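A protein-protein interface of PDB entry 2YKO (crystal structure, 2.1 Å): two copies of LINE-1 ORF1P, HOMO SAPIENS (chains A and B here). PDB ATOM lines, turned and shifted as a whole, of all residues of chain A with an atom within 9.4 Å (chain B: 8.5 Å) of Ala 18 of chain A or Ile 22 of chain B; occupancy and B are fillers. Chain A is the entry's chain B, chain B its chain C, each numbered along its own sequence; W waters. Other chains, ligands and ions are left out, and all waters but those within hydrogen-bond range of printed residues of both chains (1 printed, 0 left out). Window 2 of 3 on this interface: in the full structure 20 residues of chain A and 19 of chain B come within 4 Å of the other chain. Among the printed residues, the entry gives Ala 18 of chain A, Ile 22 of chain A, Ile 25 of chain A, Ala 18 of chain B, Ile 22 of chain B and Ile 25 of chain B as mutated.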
ATOM      1  N   LEU A  11     -14.541 -26.648  15.328  1.00  0.00           N
ATOM      2  CA  LEU A  11     -15.842 -25.993  15.268  1.00  0.00           C
ATOM      3  C   LEU A  11     -15.848 -24.882  14.223  1.00  0.00           C
ATOM      4  O   LEU A  11     -16.913 -24.473  13.765  1.00  0.00           O
ATOM      5  CB  LEU A  11     -16.241 -25.418  16.638  1.00  0.00           C
ATOM      6  N   GLU A  12     -14.665 -24.409  13.842  1.00  0.00           N
ATOM      7  CA  GLU A  12     -14.539 -23.302  12.893  1.00  0.00           C
ATOM      8  C   GLU A  12     -15.367 -23.518  11.632  1.00  0.00           C
ATOM      9  O   GLU A  12     -15.956 -22.578  11.094  1.00  0.00           O
ATOM     10  CB  GLU A  12     -13.078 -23.111  12.492  1.00  0.00           C
ATOM     11  N   GLU A  13     -15.398 -24.751  11.138  1.00  0.00           N
ATOM     12  CA  GLU A  13     -16.217 -25.053   9.973  1.00  0.00           C
ATOM     13  C   GLU A  13     -17.692 -24.748  10.280  1.00  0.00           C
ATOM     14  O   GLU A  13     -18.380 -24.113   9.470  1.00  0.00           O
ATOM     15  CB  GLU A  13     -16.022 -26.509   9.520  1.00  0.00           C
ATOM     16  N   ARG A  14     -18.163 -25.173  11.454  1.00  0.00           N
ATOM     17  CA  ARG A  14     -19.565 -24.971  11.841  1.00  0.00           C
ATOM     18  C   ARG A  14     -20.004 -23.506  11.965  1.00  0.00           C
ATOM     19  O   ARG A  14     -21.174 -23.175  11.683  1.00  0.00           O
ATOM     20  CB  ARG A  14     -19.857 -25.669  13.165  1.00  0.00           C
ATOM     21  CG  ARG A  14     -19.867 -27.175  13.065  1.00  0.00           C
ATOM     22  CD  ARG A  14     -19.879 -27.820  14.435  1.00  0.00           C
ATOM     23  NE  ARG A  14     -21.132 -27.611  15.157  1.00  0.00           N
ATOM     24  CZ  ARG A  14     -21.306 -27.917  16.440  1.00  0.00           C
ATOM     25  NH1 ARG A  14     -20.309 -28.456  17.145  1.00  0.00           N
ATOM     26  NH2 ARG A  14     -22.475 -27.690  17.024  1.00  0.00           N
ATOM     27  N   VAL A  15     -19.091 -22.649  12.424  1.00  0.00           N
ATOM     28  CA  VAL A  15     -19.380 -21.235  12.581  1.00  0.00           C
ATOM     29  C   VAL A  15     -19.405 -20.544  11.215  1.00  0.00           C
ATOM     30  O   VAL A  15     -20.241 -19.685  10.973  1.00  0.00           O
ATOM     31  CB  VAL A  15     -18.350 -20.530  13.500  1.00  0.00           C
ATOM     32  CG1 VAL A  15     -16.997 -20.475  12.855  1.00  0.00           C
ATOM     33  CG2 VAL A  15     -18.799 -19.118  13.812  1.00  0.00           C
ATOM     34  N   SER A  16     -18.479 -20.938  10.341  1.00  0.00           N
ATOM     35  CA  SER A  16     -18.361 -20.398   8.989  1.00  0.00           C
ATOM     36  C   SER A  16     -19.639 -20.717   8.223  1.00  0.00           C
ATOM     37  O   SER A  16     -20.223 -19.848   7.564  1.00  0.00           O
ATOM     38  CB  SER A  16     -17.123 -21.001   8.288  1.00  0.00           C
ATOM     39  OG  SER A  16     -16.876 -20.413   7.014  1.00  0.00           O
ATOM     40  N   ALA A  17     -20.082 -21.966   8.348  1.00  0.00           N
ATOM     41  CA  ALA A  17     -21.353 -22.406   7.790  1.00  0.00           C
ATOM     42  C   ALA A  17     -22.548 -21.616   8.356  1.00  0.00           C
ATOM     43  O   ALA A  17     -23.420 -21.180   7.586  1.00  0.00           O
ATOM     44  CB  ALA A  17     -21.545 -23.889   8.039  1.00  0.00           C
ATOM     45  N   ALA A  18     -22.597 -21.437   9.682  1.00  0.00           N
ATOM     46  CA  ALA A  18     -23.681 -20.674  10.302  1.00  0.00           C
ATOM     47  C   ALA A  18     -23.689 -19.248   9.753  1.00  0.00           C
ATOM     48  O   ALA A  18     -24.740 -18.702   9.481  1.00  0.00           O
ATOM     49  CB  ALA A  18     -23.560 -20.650  11.821  1.00  0.00           C
ATOM     50  N   GLU A  19     -22.521 -18.648   9.615  1.00  0.00           N
ATOM     51  CA  GLU A  19     -22.417 -17.320   9.027  1.00  0.00           C
ATOM     52  C   GLU A  19     -22.952 -17.328   7.602  1.00  0.00           C
ATOM     53  O   GLU A  19     -23.563 -16.361   7.179  1.00  0.00           O
ATOM     54  CB  GLU A  19     -20.961 -16.850   8.991  1.00  0.00           C
ATOM     55  CG  GLU A  19     -20.281 -16.745  10.338  1.00  0.00           C
ATOM     56  CD  GLU A  19     -18.773 -16.584  10.187  1.00  0.00           C
ATOM     57  OE1 GLU A  19     -18.192 -17.258   9.296  1.00  0.00           O
ATOM     58  OE2 GLU A  19     -18.190 -15.758  10.932  1.00  0.00           O
ATOM     59  N   ASP A  20     -22.701 -18.404   6.854  1.00  0.00           N
ATOM     60  CA  ASP A  20     -23.198 -18.502   5.483  1.00  0.00           C
ATOM     61  C   ASP A  20     -24.715 -18.557   5.527  1.00  0.00           C
ATOM     62  O   ASP A  20     -25.377 -17.941   4.704  1.00  0.00           O
ATOM     63  CB  ASP A  20     -22.685 -19.759   4.763  1.00  0.00           C
ATOM     64  CG  ASP A  20     -21.181 -19.708   4.439  1.00  0.00           C
ATOM     65  OD1 ASP A  20     -20.556 -18.636   4.594  1.00  0.00           O
ATOM     66  OD2 ASP A  20     -20.640 -20.755   4.006  1.00  0.00           O
ATOM     67  N   GLU A  21     -25.267 -19.314   6.477  1.00  0.00           N
ATOM     68  CA  GLU A  21     -26.717 -19.431   6.605  1.00  0.00           C
ATOM     69  C   GLU A  21     -27.359 -18.082   6.919  1.00  0.00           C
ATOM     70  O   GLU A  21     -28.379 -17.715   6.335  1.00  0.00           O
ATOM     71  CB  GLU A  21     -27.088 -20.439   7.694  1.00  0.00           C
ATOM     72  CG  GLU A  21     -26.674 -21.881   7.387  1.00  0.00           C
ATOM     73  CD  GLU A  21     -27.381 -22.441   6.155  1.00  0.00           C
ATOM     74  OE1 GLU A  21     -28.078 -21.680   5.453  1.00  0.00           O
ATOM     75  OE2 GLU A  21     -27.249 -23.646   5.882  1.00  0.00           O
ATOM     76  N   ILE A  22     -26.739 -17.358   7.852  1.00  0.00           N
ATOM     77  CA  ILE A  22     -27.208 -16.057   8.307  1.00  0.00           C
ATOM     78  C   ILE A  22     -27.221 -15.081   7.134  1.00  0.00           C
ATOM     79  O   ILE A  22     -28.177 -14.312   6.942  1.00  0.00           O
ATOM     80  CB  ILE A  22     -26.287 -15.518   9.438  1.00  0.00           C
ATOM     81  CG1 ILE A  22     -26.528 -16.326  10.724  1.00  0.00           C
ATOM     82  CG2 ILE A  22     -26.567 -14.059   9.702  1.00  0.00           C
ATOM     83  CD1 ILE A  22     -25.557 -16.037  11.900  1.00  0.00           C
ATOM     84  N   ASN A  23     -26.135 -15.101   6.366  1.00  0.00           N
ATOM     85  CA  ASN A  23     -26.033 -14.245   5.200  1.00  0.00           C
ATOM     86  C   ASN A  23     -27.094 -14.611   4.191  1.00  0.00           C
ATOM     87  O   ASN A  23     -27.685 -13.737   3.602  1.00  0.00           O
ATOM     88  CB  ASN A  23     -24.657 -14.334   4.556  1.00  0.00           C
ATOM     89  CG  ASN A  23     -23.624 -13.457   5.252  1.00  0.00           C
ATOM     90  OD1 ASN A  23     -23.835 -12.262   5.466  1.00  0.00           O
ATOM     91  ND2 ASN A  23     -22.493 -14.056   5.609  1.00  0.00           N
ATOM     92  N   GLU A  24     -27.338 -15.899   3.973  1.00  0.00           N
ATOM     93  CA  GLU A  24     -28.404 -16.256   3.043  1.00  0.00           C
ATOM     94  C   GLU A  24     -29.773 -15.772   3.569  1.00  0.00           C
ATOM     95  O   GLU A  24     -30.619 -15.318   2.787  1.00  0.00           O
ATOM     96  CB  GLU A  24     -28.452 -17.759   2.789  1.00  0.00           C
ATOM     97  CG  GLU A  24     -29.575 -18.193   1.833  1.00  0.00           C
ATOM     98  CD  GLU A  24     -29.617 -19.704   1.630  1.00  0.00           C
ATOM     99  OE1 GLU A  24     -28.545 -20.355   1.687  1.00  0.00           O
ATOM    100  OE2 GLU A  24     -30.727 -20.245   1.426  1.00  0.00           O
ATOM    101  N   ILE A  25     -29.998 -15.887   4.883  1.00  0.00           N
ATOM    102  CA  ILE A  25     -31.306 -15.534   5.458  1.00  0.00           C
ATOM    103  C   ILE A  25     -31.558 -14.029   5.310  1.00  0.00           C
ATOM    104  O   ILE A  25     -32.633 -13.620   4.909  1.00  0.00           O
ATOM    105  CB  ILE A  25     -31.397 -15.933   6.925  1.00  0.00           C
ATOM    106  CG1 ILE A  25     -31.470 -17.456   7.042  1.00  0.00           C
ATOM    107  CG2 ILE A  25     -32.609 -15.226   7.613  1.00  0.00           C
ATOM    108  CD1 ILE A  25     -31.271 -17.928   8.479  1.00  0.00           C
ATOM    109  N   LYS A  26     -30.549 -13.213   5.616  1.00  0.00           N
ATOM    110  CA  LYS A  26     -30.653 -11.757   5.482  1.00  0.00           C
ATOM    111  C   LYS A  26     -30.956 -11.345   4.034  1.00  0.00           C
ATOM    112  O   LYS A  26     -31.747 -10.442   3.774  1.00  0.00           O
ATOM    113  CB  LYS A  26     -29.339 -11.101   5.914  1.00  0.00           C
ATOM    114  CG  LYS A  26     -29.070 -11.123   7.405  1.00  0.00           C
ATOM    115  CD  LYS A  26     -27.624 -10.683   7.714  1.00  0.00           C
ATOM    116  CE  LYS A  26     -27.336  -9.265   7.234  1.00  0.00           C
ATOM    117  NZ  LYS A  26     -28.333  -8.289   7.784  1.00  0.00           N
ATOM    118  N   ARG A  32     -37.741 -10.805   0.123  1.00  0.00           N
ATOM    119  CA  ARG A  32     -39.097 -10.977   0.615  1.00  0.00           C
ATOM    120  C   ARG A  32     -39.677  -9.629   1.038  1.00  0.00           C
ATOM    121  O   ARG A  32     -40.821  -9.326   0.752  1.00  0.00           O
ATOM    122  CB  ARG A  32     -39.146 -11.989   1.774  1.00  0.00           C
ATOM    123  CG  ARG A  32     -39.049 -13.445   1.290  1.00  0.00           C
ATOM    124  CD  ARG A  32     -39.425 -14.446   2.374  1.00  0.00           C
ATOM    125  NE  ARG A  32     -38.489 -14.439   3.497  1.00  0.00           N
ATOM    126  CZ  ARG A  32     -37.424 -15.229   3.589  1.00  0.00           C
ATOM    127  NH1 ARG A  32     -37.139 -16.091   2.614  1.00  0.00           N
ATOM    128  NH2 ARG A  32     -36.636 -15.158   4.651  1.00  0.00           N
ATOM    129  N   ARG B  14     -22.710 -22.741  22.421  1.00  0.00           N
ATOM    130  CA  ARG B  14     -23.350 -21.550  21.880  1.00  0.00           C
ATOM    131  C   ARG B  14     -23.565 -21.719  20.369  1.00  0.00           C
ATOM    132  O   ARG B  14     -24.547 -21.229  19.827  1.00  0.00           O
ATOM    133  CB  ARG B  14     -22.529 -20.298  22.220  1.00  0.00           C
ATOM    134  CG  ARG B  14     -22.624 -19.872  23.686  1.00  0.00           C
ATOM    135  CD  ARG B  14     -21.514 -18.891  24.060  1.00  0.00           C
ATOM    136  NE  ARG B  14     -21.601 -17.665  23.270  1.00  0.00           N
ATOM    137  CZ  ARG B  14     -20.666 -16.723  23.240  1.00  0.00           C
ATOM    138  NH1 ARG B  14     -19.558 -16.842  23.971  1.00  0.00           N
ATOM    139  NH2 ARG B  14     -20.835 -15.653  22.472  1.00  0.00           N
ATOM    140  N   VAL B  15     -22.657 -22.448  19.723  1.00  0.00           N
ATOM    141  CA  VAL B  15     -22.734 -22.758  18.314  1.00  0.00           C
ATOM    142  C   VAL B  15     -23.924 -23.696  17.995  1.00  0.00           C
ATOM    143  O   VAL B  15     -24.711 -23.419  17.081  1.00  0.00           O
ATOM    144  CB  VAL B  15     -21.411 -23.340  17.842  1.00  0.00           C
ATOM    145  CG1 VAL B  15     -21.258 -24.764  18.335  1.00  0.00           C
ATOM    146  CG2 VAL B  15     -21.323 -23.319  16.358  1.00  0.00           C
ATOM    147  N   SER B  16     -24.086 -24.764  18.773  1.00  0.00           N
ATOM    148  CA  SER B  16     -25.252 -25.638  18.646  1.00  0.00           C
ATOM    149  C   SER B  16     -26.500 -24.819  18.748  1.00  0.00           C
ATOM    150  O   SER B  16     -27.339 -24.848  17.862  1.00  0.00           O
ATOM    151  CB  SER B  16     -25.278 -26.691  19.761  1.00  0.00           C
ATOM    152  OG  SER B  16     -24.126 -27.508  19.722  1.00  0.00           O
ATOM    153  N   ALA B  17     -26.635 -24.070  19.836  1.00  0.00           N
ATOM    154  CA  ALA B  17     -27.809 -23.206  19.991  1.00  0.00           C
ATOM    155  C   ALA B  17     -28.046 -22.319  18.758  1.00  0.00           C
ATOM    156  O   ALA B  17     -29.192 -22.083  18.365  1.00  0.00           O
ATOM    157  CB  ALA B  17     -27.677 -22.325  21.240  1.00  0.00           C
ATOM    158  N   ALA B  18     -26.980 -21.816  18.144  1.00  0.00           N
ATOM    159  CA  ALA B  18     -27.152 -20.875  17.024  1.00  0.00           C
ATOM    160  C   ALA B  18     -27.656 -21.636  15.794  1.00  0.00           C
ATOM    161  O   ALA B  18     -28.548 -21.178  15.094  1.00  0.00           O
ATOM    162  CB  ALA B  18     -25.854 -20.140  16.712  1.00  0.00           C
ATOM    163  N   GLU B  19     -27.097 -22.815  15.562  1.00  0.00           N
ATOM    164  CA  GLU B  19     -27.535 -23.672  14.472  1.00  0.00           C
ATOM    165  C   GLU B  19     -28.994 -24.041  14.616  1.00  0.00           C
ATOM    166  O   GLU B  19     -29.714 -24.118  13.622  1.00  0.00           O
ATOM    167  CB  GLU B  19     -26.702 -24.948  14.435  1.00  0.00           C
ATOM    168  CG  GLU B  19     -25.229 -24.721  14.108  1.00  0.00           C
ATOM    169  CD  GLU B  19     -24.384 -25.996  14.317  1.00  0.00           C
ATOM    170  OE1 GLU B  19     -24.840 -26.899  15.061  1.00  0.00           O
ATOM    171  OE2 GLU B  19     -23.267 -26.088  13.750  1.00  0.00           O
ATOM    172  N   ASP B  20     -29.449 -24.296  15.839  1.00  0.00           N
ATOM    173  CA  ASP B  20     -30.861 -24.630  16.003  1.00  0.00           C
ATOM    174  C   ASP B  20     -31.770 -23.437  15.722  1.00  0.00           C
ATOM    175  O   ASP B  20     -32.840 -23.610  15.139  1.00  0.00           O
ATOM    176  CB  ASP B  20     -31.147 -25.204  17.374  1.00  0.00           C
ATOM    177  CG  ASP B  20     -30.562 -26.588  17.538  1.00  0.00           C
ATOM    178  OD1 ASP B  20     -30.172 -27.189  16.510  1.00  0.00           O
ATOM    179  OD2 ASP B  20     -30.485 -27.076  18.680  1.00  0.00           O
ATOM    180  N   GLU B  21     -31.356 -22.236  16.128  1.00  0.00           N
ATOM    181  CA  GLU B  21     -32.185 -21.059  15.907  1.00  0.00           C
ATOM    182  C   GLU B  21     -32.263 -20.755  14.408  1.00  0.00           C
ATOM    183  O   GLU B  21     -33.278 -20.294  13.910  1.00  0.00           O
ATOM    184  CB  GLU B  21     -31.621 -19.853  16.655  1.00  0.00           C
ATOM    185  CG  GLU B  21     -32.160 -19.689  18.092  1.00  0.00           C
ATOM    186  CD  GLU B  21     -33.526 -19.012  18.141  1.00  0.00           C
ATOM    187  OE1 GLU B  21     -34.432 -19.408  17.369  1.00  0.00           O
ATOM    188  OE2 GLU B  21     -33.693 -18.065  18.945  1.00  0.00           O
ATOM    189  N   ILE B  22     -31.162 -21.023  13.714  1.00  0.00           N
ATOM    190  CA  ILE B  22     -31.069 -20.806  12.293  1.00  0.00           C
ATOM    191  C   ILE B  22     -32.075 -21.687  11.562  1.00  0.00           C
ATOM    192  O   ILE B  22     -32.742 -21.245  10.619  1.00  0.00           O
ATOM    193  CB  ILE B  22     -29.640 -21.084  11.820  1.00  0.00           C
ATOM    194  CG1 ILE B  22     -28.771 -19.855  12.119  1.00  0.00           C
ATOM    195  CG2 ILE B  22     -29.600 -21.444  10.325  1.00  0.00           C
ATOM    196  CD1 ILE B  22     -27.245 -20.112  11.922  1.00  0.00           C
ATOM    197  N   ASN B  23     -32.207 -22.927  12.006  1.00  0.00           N
ATOM    198  CA  ASN B  23     -33.154 -23.840  11.374  1.00  0.00           C
ATOM    199  C   ASN B  23     -34.576 -23.397  11.578  1.00  0.00           C
ATOM    200  O   ASN B  23     -35.419 -23.582  10.720  1.00  0.00           O
ATOM    201  CB  ASN B  23     -32.966 -25.268  11.908  1.00  0.00           C
ATOM    202  CG  ASN B  23     -31.830 -25.986  11.224  1.00  0.00           C
ATOM    203  OD1 ASN B  23     -31.650 -25.851   9.994  1.00  0.00           O
ATOM    204  ND2 ASN B  23     -31.038 -26.748  12.003  1.00  0.00           N
ATOM    205  N   GLU B  24     -34.864 -22.809  12.725  1.00  0.00           N
ATOM    206  CA  GLU B  24     -36.223 -22.364  12.969  1.00  0.00           C
ATOM    207  C   GLU B  24     -36.589 -21.190  12.056  1.00  0.00           C
ATOM    208  O   GLU B  24     -37.688 -21.147  11.504  1.00  0.00           O
ATOM    209  CB  GLU B  24     -36.396 -21.967  14.434  1.00  0.00           C
ATOM    210  CG  GLU B  24     -37.849 -21.630  14.781  1.00  0.00           C
ATOM    211  CD  GLU B  24     -38.757 -22.856  14.793  1.00  0.00           C
ATOM    212  OE1 GLU B  24     -38.253 -23.979  15.061  1.00  0.00           O
ATOM    213  OE2 GLU B  24     -39.970 -22.688  14.522  1.00  0.00           O
ATOM    214  N   ILE B  25     -35.662 -20.240  11.931  1.00  0.00           N
ATOM    215  CA  ILE B  25     -35.810 -19.046  11.075  1.00  0.00           C
ATOM    216  C   ILE B  25     -35.955 -19.390   9.568  1.00  0.00           C
ATOM    217  O   ILE B  25     -36.772 -18.812   8.870  1.00  0.00           O
ATOM    218  CB  ILE B  25     -34.569 -18.148  11.230  1.00  0.00           C
ATOM    219  CG1 ILE B  25     -34.563 -17.503  12.623  1.00  0.00           C
ATOM    220  CG2 ILE B  25     -34.527 -17.117  10.139  1.00  0.00           C
ATOM    221  CD1 ILE B  25     -33.265 -16.778  12.974  1.00  0.00           C
ATOM    222  N   LYS B  26     -35.142 -20.324   9.076  1.00  0.00           N
ATOM    223  CA  LYS B  26     -35.292 -20.809   7.700  1.00  0.00           C
ATOM    224  C   LYS B  26     -36.695 -21.320   7.414  1.00  0.00           C
ATOM    225  O   LYS B  26     -37.259 -20.972   6.405  1.00  0.00           O
ATOM    226  CB  LYS B  26     -34.319 -21.932   7.411  1.00  0.00           C
ATOM    227  CG  LYS B  26     -32.965 -21.459   6.959  1.00  0.00           C
ATOM    228  CD  LYS B  26     -32.141 -22.648   6.508  1.00  0.00           C
ATOM    229  CE  LYS B  26     -30.909 -22.242   5.743  1.00  0.00           C
ATOM    230  NZ  LYS B  26     -30.135 -23.463   5.360  1.00  0.00           N
ATOM    231  N   ARG B  27     -37.243 -22.143   8.298  1.00  0.00           N
ATOM    232  CA  ARG B  27     -38.600 -22.648   8.121  1.00  0.00           C
ATOM    233  C   ARG B  27     -39.644 -21.554   8.215  1.00  0.00           C
ATOM    234  O   ARG B  27     -40.569 -21.522   7.410  1.00  0.00           O
ATOM    235  CB  ARG B  27     -38.935 -23.722   9.160  1.00  0.00           C
ATOM    236  CG  ARG B  27     -38.209 -25.020   8.957  1.00  0.00           C
ATOM    237  CD  ARG B  27     -38.853 -26.088   9.805  1.00  0.00           C
ATOM    238  NE  ARG B  27     -38.416 -26.071  11.199  1.00  0.00           N
ATOM    239  CZ  ARG B  27     -37.503 -26.911  11.692  1.00  0.00           C
ATOM    240  NH1 ARG B  27     -36.914 -27.804  10.901  1.00  0.00           N
ATOM    241  NH2 ARG B  27     -37.160 -26.866  12.974  1.00  0.00           N
ATOM    242  N   GLU B  28     -39.518 -20.673   9.216  1.00  0.00           N
ATOM    243  CA  GLU B  28     -40.458 -19.573   9.337  1.00  0.00           C
ATOM    244  C   GLU B  28     -40.392 -18.763   8.046  1.00  0.00           C
ATOM    245  O   GLU B  28     -41.402 -18.317   7.510  1.00  0.00           O
ATOM    246  CB  GLU B  28     -40.131 -18.648  10.516  1.00  0.00           C
ATOM    247  CG  GLU B  28     -40.856 -18.981  11.813  1.00  0.00           C
ATOM    248  CD  GLU B  28     -42.363 -19.172  11.631  1.00  0.00           C
ATOM    249  OE1 GLU B  28     -43.098 -18.166  11.415  1.00  0.00           O
ATOM    250  OE2 GLU B  28     -42.809 -20.335  11.720  1.00  0.00           O
ATOM    251  N   GLY B  29     -39.182 -18.563   7.558  1.00  0.00           N
ATOM    252  CA  GLY B  29     -38.979 -17.726   6.391  1.00  0.00           C
ATOM    253  C   GLY B  29     -39.653 -18.331   5.164  1.00  0.00           C
ATOM    254  O   GLY B  29     -40.282 -17.624   4.386  1.00  0.00           O
HETATM  255  O   HOH W   1     -35.902 -16.877   7.009  1.00  0.00           O
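The side-chain carboxylate (OE1) of Glu 21 of chain A is in salt-bridge range of the side-chain amino group (NZ) of Lys 26 of chain B, 2.7 Å away. The side-chain hydroxyl (OG) of Ser 16 of chain B sits at hydrogen-bond distance from the guanidinium group (NH2) of Arg 14 of chain A (3.2 Å). The guanidinium group (NE) of Arg 14 of chain A lies within salt-bridge range of the side-chain carboxylate (OE2) of Glu 19 of chain B (3.0 Å).
The side-chain amide nitrogen (ND2) of Asn 23 of chain B is in hydrogen-bond range of the backbone carbonyl oxygen (O) of Glu 19 of chain B (3.4 Å).
Among the printed residues, merely in contact across the chains: Arg 14 of chain A with Val 15 of chain B (3.4 Å), Ile 25 of chain A with Ile 25 of chain B (3.7 Å), Ala 18 of chain A with Ile 22 of chain B (3.7 Å), Arg 32 of chain A with Gly 29 of chain B (3.8 Å) and Glu 21 of chain A with Ile 22 of chain B (3.8 Å).
Of the printed residues of chain B, Glu 21 of chain A touches Ile 22 (3.8 Å) and Lys 26 (2.7 Å). Of the printed residues of chain B, Ile 25 of chain A touches Ile 25 (3.7 Å). Of the printed residues of chain A, Ser 16 of chain B touches Arg 14 (3.2 Å). Ile 22 of chain B touches just these residues of chain A: Ala 18 and Glu 21. No residue of chain A comes within 4 Å of Asn 23 of chain B. Ile 25 of chain B touches just one residue of chain A: Ile 25 (3.7 Å). Printed residues of chain A within 4 Å of Gly 29 of chain B: Arg 32 (3.8 Å). The nearest residue of chain B that does not touch Ala 18 of chain A is Glu 19 of chain B (5.0 Å). The nearest residue of chain A that does not touch Ile 22 of chain B is Ile 22 of chain A (4.04 Å). The nearest printed residue of chain A that does not touch Val 15 of chain B is Val 15 of chain A (4.6 Å).
Hydrophobic or aromatic side chains of chain A that line the printed part of chain B: Ala 18 and Ile 25. Along chain B the printed residues that touch a printed residue of chain A span positions 15 to 29. Among the printed residues, 8 pairs touch across the chains. Among the printed residues, Asp or Glu carboxylates within 4 Å of a Lys or Arg side-chain nitrogen of the other chain: Arg 14 of chain A with Glu 19 of chain B and Glu 21 of chain A with Lys 26 of chain B.
Arg 14 of chain A touches Ser 16 of chain B, but with the chains exchanged Ser 16 of chain A does not touch Arg 14 of chain B (11.3 Å). Ala 18 of chain A touches Ile 22 of chain B, but with the chains exchanged Ile 22 of chain A does not touch Ala 18 of chain B (6.3 Å). Glu 21 of chain A touches Lys 26 of chain B, but with the chains exchanged Lys 26 of chain A does not touch Glu 21 of chain B (11.2 Å). Ile 25 of chain B touches its own counterpart, Ile 25 of chain A. Of the 8 pairs that touch across the chains among the printed residues, 1 has its exchanged pair printed and touching as well.
Water W1 bridges the backbone carbonyl oxygen (O) of Ile 25 of chain B (2.8 Å) and the guanidinium group (NH2) of Arg 32 of chain A (3.0 Å).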
